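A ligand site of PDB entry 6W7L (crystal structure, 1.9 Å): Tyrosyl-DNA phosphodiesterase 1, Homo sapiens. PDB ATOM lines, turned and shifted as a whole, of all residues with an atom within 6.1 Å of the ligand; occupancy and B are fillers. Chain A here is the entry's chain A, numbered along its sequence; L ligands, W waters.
The side-chain amide nitrogen of Asn 369 is in hydrogen-bond range of an oxygen (O2) of the ligand.
O3 of the ligand sits at hydrogen-bond distance from ND1 of His 116 (2.8 Å).
A nitrogen (N1) of the ligand is in hydrogen-bond range of the side-chain hydroxyl of Tyr 57 (3.1 Å).
ND2 of Asn 136 is in hydrogen-bond range of O4 of the ligand, at 3.0 Å.
A ring nitrogen (NE2) of His 346 lies within hydrogen-bond range of an oxygen (O4) of the ligand, at 2.9 Å.
The side-chain amino group of Lys 118 lies within salt-bridge range of an oxygen (O3) of the ligand, at 2.6 Å.
The side-chain amino group of Lys 348 is in salt-bridge range of an oxygen (O2) of the ligand, at 2.7 Å.
O1 of the ligand lies within hydrogen-bond range of OG of Ser 252, at 2.8 Å.
Thr 114 touches the ligand.
CB of Ser 253 touches O1 of the ligand, 3.8 Å away.
Pro 314 touches the ligand (CG to C10, 3.3 Å).
Trp 443 touches the ligand.
Hydrophobic or aromatic side chains within 4 Å of the ligand: Tyr 57, His 116, Pro 314, His 346 and Trp 443.
Of the 23 residues printed, 12 come within 4 Å of the ligand.
The nearest printed residue that does not touch the ligand is Ser 312 (4.3 Å).
The backbone carbonyl oxygen (O) of Pro 314 is in hydrogen-bond range of the side-chain hydroxyl (OG) of Ser 253, at 2.8 Å.
N of Ser 252 sits at hydrogen-bond distance from OD1 of Asn 369 (3.0 Å).
The side-chain amino group (NZ) of Lys 348 sits at hydrogen-bond distance from the side-chain hydroxyl (OG) of Ser 252 (3.1 Å).
The side-chain amide oxygen (OD1) of Asn 56 sits close to the side-chain amide oxygen (OD1) of Asn 136, 3.0 Å away.
NZ of Lys 348 is in hydrogen-bond range of O of His 346, at 2.9 Å.
The side-chain amide oxygen (OD1) of Asn 369 lies within hydrogen-bond range of the backbone NH (N) of Ser 253 (3.1 Å).
The backbone carbonyl oxygen of Thr 134 is in hydrogen-bond range of a ring nitrogen (ND1) of His 346 (2.8 Å).
N of Asn 136 lies within hydrogen-bond range of OD2 of Asp 141 (2.9 Å).
Water W3 lies within hydrogen-bond range of an oxygen (O2) of the ligand (2.6 Å), the backbone carbonyl oxygen (O) of Ser 367 (2.8 Å), the side-chain amino group (NZ) of Lys 348 (3.3 Å), the side-chain amino group (NZ) of Lys 118 (3.3 Å) and a ring nitrogen (ND1) of His 116 (3.4 Å).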
ATOM      1  N   ASN A  56      -3.656  -3.295 -36.182  1.00  0.00           N
ATOM      2  CA  ASN A  56      -4.762  -3.190 -35.244  1.00  0.00           C
ATOM      3  C   ASN A  56      -4.435  -3.931 -33.944  1.00  0.00           C
ATOM      4  O   ASN A  56      -3.342  -4.473 -33.767  1.00  0.00           O
ATOM      5  CB  ASN A  56      -6.079  -3.689 -35.873  1.00  0.00           C
ATOM      6  CG  ASN A  56      -7.288  -2.834 -35.450  1.00  0.00           C
ATOM      7  OD1 ASN A  56      -7.704  -2.914 -34.309  1.00  0.00           O
ATOM      8  ND2 ASN A  56      -7.846  -2.025 -36.382  1.00  0.00           N
ATOM      9  N   TYR A  57      -5.411  -3.908 -33.038  1.00  0.00           N
ATOM     10  CA  TYR A  57      -5.385  -4.646 -31.777  1.00  0.00           C
ATOM     11  C   TYR A  57      -6.141  -5.968 -31.851  1.00  0.00           C
ATOM     12  O   TYR A  57      -5.573  -7.026 -31.529  1.00  0.00           O
ATOM     13  CB  TYR A  57      -5.962  -3.782 -30.646  1.00  0.00           C
ATOM     14  CG  TYR A  57      -6.105  -4.577 -29.369  1.00  0.00           C
ATOM     15  CD1 TYR A  57      -4.991  -4.913 -28.619  1.00  0.00           C
ATOM     16  CD2 TYR A  57      -7.352  -5.053 -28.955  1.00  0.00           C
ATOM     17  CE1 TYR A  57      -5.105  -5.688 -27.469  1.00  0.00           C
ATOM     18  CE2 TYR A  57      -7.471  -5.842 -27.815  1.00  0.00           C
ATOM     19  CZ  TYR A  57      -6.351  -6.141 -27.075  1.00  0.00           C
ATOM     20  OH  TYR A  57      -6.455  -6.902 -25.939  1.00  0.00           O
ATOM     21  N   CYS A  58      -7.407  -5.943 -32.258  1.00  0.00           N
ATOM     22  CA  CYS A  58      -8.279  -7.111 -32.311  1.00  0.00           C
ATOM     23  C   CYS A  58      -8.707  -7.358 -33.753  1.00  0.00           C
ATOM     24  O   CYS A  58      -8.991  -6.403 -34.486  1.00  0.00           O
ATOM     25  CB  CYS A  58      -9.548  -6.926 -31.413  1.00  0.00           C
ATOM     26  SG  CYS A  58     -10.467  -8.438 -31.121  1.00  0.00           S
ATOM     27  N   PHE A 112       3.474  -5.041 -19.976  1.00  0.00           N
ATOM     28  CA  PHE A 112       2.159  -4.416 -19.905  1.00  0.00           C
ATOM     29  C   PHE A 112       1.916  -3.425 -21.057  1.00  0.00           C
ATOM     30  O   PHE A 112       1.123  -2.496 -20.921  1.00  0.00           O
ATOM     31  CB  PHE A 112       1.934  -3.738 -18.544  1.00  0.00           C
ATOM     32  CG  PHE A 112       2.222  -4.633 -17.359  1.00  0.00           C
ATOM     33  CD1 PHE A 112       1.510  -5.808 -17.182  1.00  0.00           C
ATOM     34  CD2 PHE A 112       3.199  -4.298 -16.434  1.00  0.00           C
ATOM     35  CE1 PHE A 112       1.759  -6.633 -16.085  1.00  0.00           C
ATOM     36  CE2 PHE A 112       3.456  -5.116 -15.339  1.00  0.00           C
ATOM     37  CZ  PHE A 112       2.734  -6.283 -15.169  1.00  0.00           C
ATOM     38  N   GLY A 113       2.577  -3.620 -22.191  1.00  0.00           N
ATOM     39  CA  GLY A 113       2.311  -2.832 -23.370  1.00  0.00           C
ATOM     40  C   GLY A 113       1.340  -3.528 -24.313  1.00  0.00           C
ATOM     41  O   GLY A 113       1.047  -4.711 -24.207  1.00  0.00           O
ATOM     42  N   THR A 114       0.859  -2.764 -25.277  1.00  0.00           N
ATOM     43  CA  THR A 114      -0.199  -3.196 -26.168  1.00  0.00           C
ATOM     44  C   THR A 114       0.071  -2.586 -27.537  1.00  0.00           C
ATOM     45  O   THR A 114       0.649  -1.515 -27.640  1.00  0.00           O
ATOM     46  CB  THR A 114      -1.582  -2.735 -25.657  1.00  0.00           C
ATOM     47  OG1 THR A 114      -1.831  -3.300 -24.356  1.00  0.00           O
ATOM     48  CG2 THR A 114      -2.695  -3.198 -26.594  1.00  0.00           C
ATOM     49  N   HIS A 115      -0.328  -3.295 -28.585  1.00  0.00           N
ATOM     50  CA  HIS A 115      -0.295  -2.711 -29.922  1.00  0.00           C
ATOM     51  C   HIS A 115      -1.690  -2.168 -30.244  1.00  0.00           C
ATOM     52  O   HIS A 115      -2.569  -2.902 -30.711  1.00  0.00           O
ATOM     53  CB  HIS A 115       0.176  -3.740 -30.940  1.00  0.00           C
ATOM     54  CG  HIS A 115       0.304  -3.179 -32.324  1.00  0.00           C
ATOM     55  ND1 HIS A 115      -0.741  -3.173 -33.210  1.00  0.00           N
ATOM     56  CD2 HIS A 115       1.337  -2.561 -32.938  1.00  0.00           C
ATOM     57  CE1 HIS A 115      -0.345  -2.589 -34.339  1.00  0.00           C
ATOM     58  NE2 HIS A 115       0.916  -2.209 -34.199  1.00  0.00           N
ATOM     59  N   HIS A 116      -1.893  -0.862 -29.966  1.00  0.00           N
ATOM     60  CA  HIS A 116      -3.194  -0.202 -30.164  1.00  0.00           C
ATOM     61  C   HIS A 116      -3.338   0.483 -31.514  1.00  0.00           C
ATOM     62  O   HIS A 116      -4.463   0.820 -31.908  1.00  0.00           O
ATOM     63  CB  HIS A 116      -3.466   0.880 -29.120  1.00  0.00           C
ATOM     64  CG  HIS A 116      -3.727   0.381 -27.735  1.00  0.00           C
ATOM     65  ND1 HIS A 116      -4.919  -0.187 -27.348  1.00  0.00           N
ATOM     66  CD2 HIS A 116      -2.962   0.453 -26.612  1.00  0.00           C
ATOM     67  CE1 HIS A 116      -4.866  -0.496 -26.066  1.00  0.00           C
ATOM     68  NE2 HIS A 116      -3.693  -0.102 -25.593  1.00  0.00           N
ATOM     69  N   LYS A 118      -4.096   1.682 -35.068  1.00  0.00           N
ATOM     70  CA  LYS A 118      -5.117   1.266 -36.025  1.00  0.00           C
ATOM     71  C   LYS A 118      -4.907   2.065 -37.304  1.00  0.00           C
ATOM     72  O   LYS A 118      -5.118   3.289 -37.329  1.00  0.00           O
ATOM     73  CB  LYS A 118      -6.515   1.447 -35.432  1.00  0.00           C
ATOM     74  CG  LYS A 118      -6.672   0.512 -34.182  1.00  0.00           C
ATOM     75  CD  LYS A 118      -7.956   0.801 -33.474  1.00  0.00           C
ATOM     76  CE  LYS A 118      -8.142  -0.102 -32.265  1.00  0.00           C
ATOM     77  NZ  LYS A 118      -7.149   0.234 -31.238  1.00  0.00           N
ATOM     78  N   THR A 134      -9.742   4.485 -35.601  1.00  0.00           N
ATOM     79  CA  THR A 134      -9.868   4.115 -34.203  1.00  0.00           C
ATOM     80  C   THR A 134     -10.599   2.788 -33.967  1.00  0.00           C
ATOM     81  O   THR A 134     -10.723   2.389 -32.808  1.00  0.00           O
ATOM     82  CB  THR A 134     -10.565   5.236 -33.394  1.00  0.00           C
ATOM     83  OG1 THR A 134     -11.938   5.329 -33.789  1.00  0.00           O
ATOM     84  CG2 THR A 134      -9.922   6.609 -33.627  1.00  0.00           C
ATOM     85  N   ASN A 136     -11.353  -1.357 -34.004  1.00  0.00           N
ATOM     86  CA  ASN A 136     -10.847  -2.719 -34.172  1.00  0.00           C
ATOM     87  C   ASN A 136     -11.512  -3.342 -35.394  1.00  0.00           C
ATOM     88  O   ASN A 136     -12.549  -2.870 -35.864  1.00  0.00           O
ATOM     89  CB  ASN A 136     -11.123  -3.563 -32.925  1.00  0.00           C
ATOM     90  CG  ASN A 136     -10.307  -3.107 -31.751  1.00  0.00           C
ATOM     91  OD1 ASN A 136      -9.118  -3.408 -31.656  1.00  0.00           O
ATOM     92  ND2 ASN A 136     -10.918  -2.326 -30.870  1.00  0.00           N
ATOM     93  N   ASP A 141     -17.255  -3.067 -33.630  1.00  0.00           N
ATOM     94  CA  ASP A 141     -16.630  -1.744 -33.603  1.00  0.00           C
ATOM     95  C   ASP A 141     -17.102  -0.870 -34.754  1.00  0.00           C
ATOM     96  O   ASP A 141     -16.896   0.344 -34.709  1.00  0.00           O
ATOM     97  CB  ASP A 141     -15.092  -1.870 -33.635  1.00  0.00           C
ATOM     98  CG  ASP A 141     -14.486  -1.800 -32.229  1.00  0.00           C
ATOM     99  OD1 ASP A 141     -15.093  -2.391 -31.301  1.00  0.00           O
ATOM    100  OD2 ASP A 141     -13.451  -1.129 -32.027  1.00  0.00           O
ATOM    101  N   SER A 252     -11.756   6.190 -24.381  1.00  0.00           N
ATOM    102  CA  SER A 252     -12.565   5.031 -24.040  1.00  0.00           C
ATOM    103  C   SER A 252     -11.986   4.169 -22.927  1.00  0.00           C
ATOM    104  O   SER A 252     -12.669   3.233 -22.488  1.00  0.00           O
ATOM    105  CB  SER A 252     -12.792   4.133 -25.282  1.00  0.00           C
ATOM    106  OG  SER A 252     -11.555   3.805 -25.891  1.00  0.00           O
ATOM    107  N   SER A 253     -10.767   4.461 -22.447  1.00  0.00           N
ATOM    108  CA  SER A 253     -10.177   3.658 -21.389  1.00  0.00           C
ATOM    109  C   SER A 253      -9.292   4.547 -20.528  1.00  0.00           C
ATOM    110  O   SER A 253      -8.797   5.598 -20.975  1.00  0.00           O
ATOM    111  CB  SER A 253      -9.389   2.470 -21.969  1.00  0.00           C
ATOM    112  OG  SER A 253      -8.644   1.792 -20.990  1.00  0.00           O
ATOM    113  N   GLY A 311     -18.326  -3.421 -22.653  1.00  0.00           N
ATOM    114  CA  GLY A 311     -17.245  -4.349 -22.927  1.00  0.00           C
ATOM    115  C   GLY A 311     -16.108  -3.747 -23.729  1.00  0.00           C
ATOM    116  O   GLY A 311     -15.024  -4.334 -23.777  1.00  0.00           O
ATOM    117  N   SER A 312     -16.329  -2.595 -24.365  1.00  0.00           N
ATOM    118  CA  SER A 312     -15.275  -1.853 -25.073  1.00  0.00           C
ATOM    119  C   SER A 312     -14.930  -0.532 -24.398  1.00  0.00           C
ATOM    120  O   SER A 312     -14.392   0.367 -25.065  1.00  0.00           O
ATOM    121  CB  SER A 312     -15.643  -1.598 -26.532  1.00  0.00           C
ATOM    122  OG  SER A 312     -16.130  -2.760 -27.153  1.00  0.00           O
ATOM    123  N   LEU A 313     -15.264  -0.376 -23.110  1.00  0.00           N
ATOM    124  CA  LEU A 313     -14.822   0.757 -22.303  1.00  0.00           C
ATOM    125  C   LEU A 313     -14.110   0.152 -21.093  1.00  0.00           C
ATOM    126  O   LEU A 313     -14.702   0.047 -19.995  1.00  0.00           O
ATOM    127  CB  LEU A 313     -16.004   1.639 -21.888  1.00  0.00           C
ATOM    128  CG  LEU A 313     -16.804   2.265 -23.032  1.00  0.00           C
ATOM    129  CD1 LEU A 313     -18.219   2.617 -22.559  1.00  0.00           C
ATOM    130  CD2 LEU A 313     -16.088   3.505 -23.611  1.00  0.00           C
ATOM    131  N   PRO A 314     -12.865  -0.300 -21.264  1.00  0.00           N
ATOM    132  CA  PRO A 314     -12.206  -1.051 -20.185  1.00  0.00           C
ATOM    133  C   PRO A 314     -11.576  -0.117 -19.162  1.00  0.00           C
ATOM    134  O   PRO A 314     -10.562   0.544 -19.402  1.00  0.00           O
ATOM    135  CB  PRO A 314     -11.161  -1.903 -20.910  1.00  0.00           C
ATOM    136  CG  PRO A 314     -10.859  -1.161 -22.121  1.00  0.00           C
ATOM    137  CD  PRO A 314     -12.076  -0.338 -22.509  1.00  0.00           C
ATOM    138  N   HIS A 346     -15.627   4.963 -29.123  1.00  0.00           N
ATOM    139  CA  HIS A 346     -14.349   4.286 -29.109  1.00  0.00           C
ATOM    140  C   HIS A 346     -13.284   5.125 -29.793  1.00  0.00           C
ATOM    141  O   HIS A 346     -12.105   4.757 -29.763  1.00  0.00           O
ATOM    142  CB  HIS A 346     -14.483   2.898 -29.781  1.00  0.00           C
ATOM    143  CG  HIS A 346     -13.276   2.017 -29.618  1.00  0.00           C
ATOM    144  ND1 HIS A 346     -12.321   1.872 -30.611  1.00  0.00           N
ATOM    145  CD2 HIS A 346     -12.875   1.238 -28.583  1.00  0.00           C
ATOM    146  CE1 HIS A 346     -11.384   1.039 -30.184  1.00  0.00           C
ATOM    147  NE2 HIS A 346     -11.697   0.645 -28.965  1.00  0.00           N
ATOM    148  N   LYS A 348     -10.821   8.343 -29.803  1.00  0.00           N
ATOM    149  CA  LYS A 348     -10.124   9.170 -28.814  1.00  0.00           C
ATOM    150  C   LYS A 348      -9.737  10.472 -29.469  1.00  0.00           C
ATOM    151  O   LYS A 348      -9.254  10.471 -30.609  1.00  0.00           O
ATOM    152  CB  LYS A 348      -8.867   8.505 -28.247  1.00  0.00           C
ATOM    153  CG  LYS A 348      -9.123   7.179 -27.523  1.00  0.00           C
ATOM    154  CD  LYS A 348      -9.142   6.032 -28.551  1.00  0.00           C
ATOM    155  CE  LYS A 348      -8.862   4.693 -27.908  1.00  0.00           C
ATOM    156  NZ  LYS A 348      -9.781   3.696 -28.465  1.00  0.00           N
ATOM    157  N   SER A 367      -5.361   6.682 -31.382  1.00  0.00           N
ATOM    158  CA  SER A 367      -5.675   5.483 -30.617  1.00  0.00           C
ATOM    159  C   SER A 367      -5.308   5.617 -29.129  1.00  0.00           C
ATOM    160  O   SER A 367      -5.693   4.747 -28.336  1.00  0.00           O
ATOM    161  CB  SER A 367      -4.949   4.264 -31.220  1.00  0.00           C
ATOM    162  OG  SER A 367      -3.525   4.436 -31.177  1.00  0.00           O
ATOM    163  N   ASN A 369      -5.355   6.300 -25.355  1.00  0.00           N
ATOM    164  CA  ASN A 369      -6.262   6.521 -24.235  1.00  0.00           C
ATOM    165  C   ASN A 369      -5.590   7.357 -23.150  1.00  0.00           C
ATOM    166  O   ASN A 369      -4.454   7.795 -23.291  1.00  0.00           O
ATOM    167  CB  ASN A 369      -6.739   5.179 -23.677  1.00  0.00           C
ATOM    168  CG  ASN A 369      -7.881   4.617 -24.461  1.00  0.00           C
ATOM    169  OD1 ASN A 369      -8.871   5.314 -24.697  1.00  0.00           O
ATOM    170  ND2 ASN A 369      -7.735   3.382 -24.937  1.00  0.00           N
ATOM    171  N   TRP A 443     -16.017  -1.480 -15.947  1.00  0.00           N
ATOM    172  CA  TRP A 443     -16.558  -2.595 -16.738  1.00  0.00           C
ATOM    173  C   TRP A 443     -16.689  -3.907 -15.984  1.00  0.00           C
ATOM    174  O   TRP A 443     -17.382  -4.805 -16.468  1.00  0.00           O
ATOM    175  CB  TRP A 443     -15.730  -2.824 -18.011  1.00  0.00           C
ATOM    176  CG  TRP A 443     -14.359  -3.415 -17.833  1.00  0.00           C
ATOM    177  CD1 TRP A 443     -13.592  -3.422 -16.717  1.00  0.00           C
ATOM    178  CD2 TRP A 443     -13.585  -4.082 -18.851  1.00  0.00           C
ATOM    179  NE1 TRP A 443     -12.400  -4.059 -16.958  1.00  0.00           N
ATOM    180  CE2 TRP A 443     -12.365  -4.470 -18.261  1.00  0.00           C
ATOM    181  CE3 TRP A 443     -13.799  -4.372 -20.204  1.00  0.00           C
ATOM    182  CZ2 TRP A 443     -11.369  -5.150 -18.966  1.00  0.00           C
ATOM    183  CZ3 TRP A 443     -12.807  -5.060 -20.898  1.00  0.00           C
ATOM    184  CH2 TRP A 443     -11.606  -5.434 -20.278  1.00  0.00           C
HETATM  185  C1  LIG L   1      -7.709  -5.395 -22.567  1.00  0.00           C
HETATM  186  C2  LIG L   1     -10.406  -7.752 -23.433  1.00  0.00           C
HETATM  187  C3  LIG L   1     -10.961  -5.586 -24.288  1.00  0.00           C
HETATM  188  C4  LIG L   1      -3.852  -3.418 -21.334  1.00  0.00           C
HETATM  189  C5  LIG L   1      -4.702  -3.551 -22.419  1.00  0.00           C
HETATM  190  C6  LIG L   1      -7.516  -2.528 -26.317  1.00  0.00           C
HETATM  191  C7  LIG L   1      -8.182  -1.057 -28.217  1.00  0.00           C
HETATM  192  C8  LIG L   1      -9.232   0.897 -26.159  1.00  0.00           C
HETATM  193  C9  LIG L   1      -8.569  -0.425 -25.763  1.00  0.00           C
HETATM  194  C10 LIG L   1      -8.459  -0.741 -24.406  1.00  0.00           C
HETATM  195  C11 LIG L   1      -7.884  -1.945 -24.012  1.00  0.00           C
HETATM  196  C12 LIG L   1      -7.429  -2.835 -24.961  1.00  0.00           C
HETATM  197  C13 LIG L   1      -6.793  -4.565 -23.207  1.00  0.00           C
HETATM  198  C14 LIG L   1      -8.899  -5.920 -23.096  1.00  0.00           C
HETATM  199  C15 LIG L   1      -9.221  -7.255 -22.915  1.00  0.00           C
HETATM  200  C16 LIG L   1     -11.283  -6.922 -24.106  1.00  0.00           C
HETATM  201  C17 LIG L   1      -9.780  -5.089 -23.779  1.00  0.00           C
HETATM  202  C18 LIG L   1      -6.113  -4.895 -21.185  1.00  0.00           C
HETATM  203  C19 LIG L   1      -5.258  -4.756 -20.069  1.00  0.00           C
HETATM  204  C20 LIG L   1      -8.091  -1.323 -26.711  1.00  0.00           C
HETATM  205  N1  LIG L   1      -6.810  -4.090 -24.587  1.00  0.00           N
HETATM  206  N2  LIG L   1      -7.271  -5.570 -21.331  1.00  0.00           N
HETATM  207  N3  LIG L   1      -4.152  -4.021 -20.188  1.00  0.00           N
HETATM  208  N4  LIG L   1      -5.822  -4.292 -22.316  1.00  0.00           N
HETATM  209  O1  LIG L   1     -10.252   1.305 -25.518  1.00  0.00           O
HETATM  210  O2  LIG L   1      -8.802   1.583 -27.122  1.00  0.00           O
HETATM  211  O3  LIG L   1      -7.108  -0.977 -28.885  1.00  0.00           O
HETATM  212  O4  LIG L   1      -9.296  -0.911 -28.768  1.00  0.00           O
HETATM  213  O   HOH W   1      -2.655  -5.674 -23.810  1.00  0.00           O
HETATM  214  O   HOH W   2      -8.373  -7.264 -19.404  1.00  0.00           O
HETATM  215  O   HOH W   3      -6.823   2.250 -28.647  1.00  0.00           O
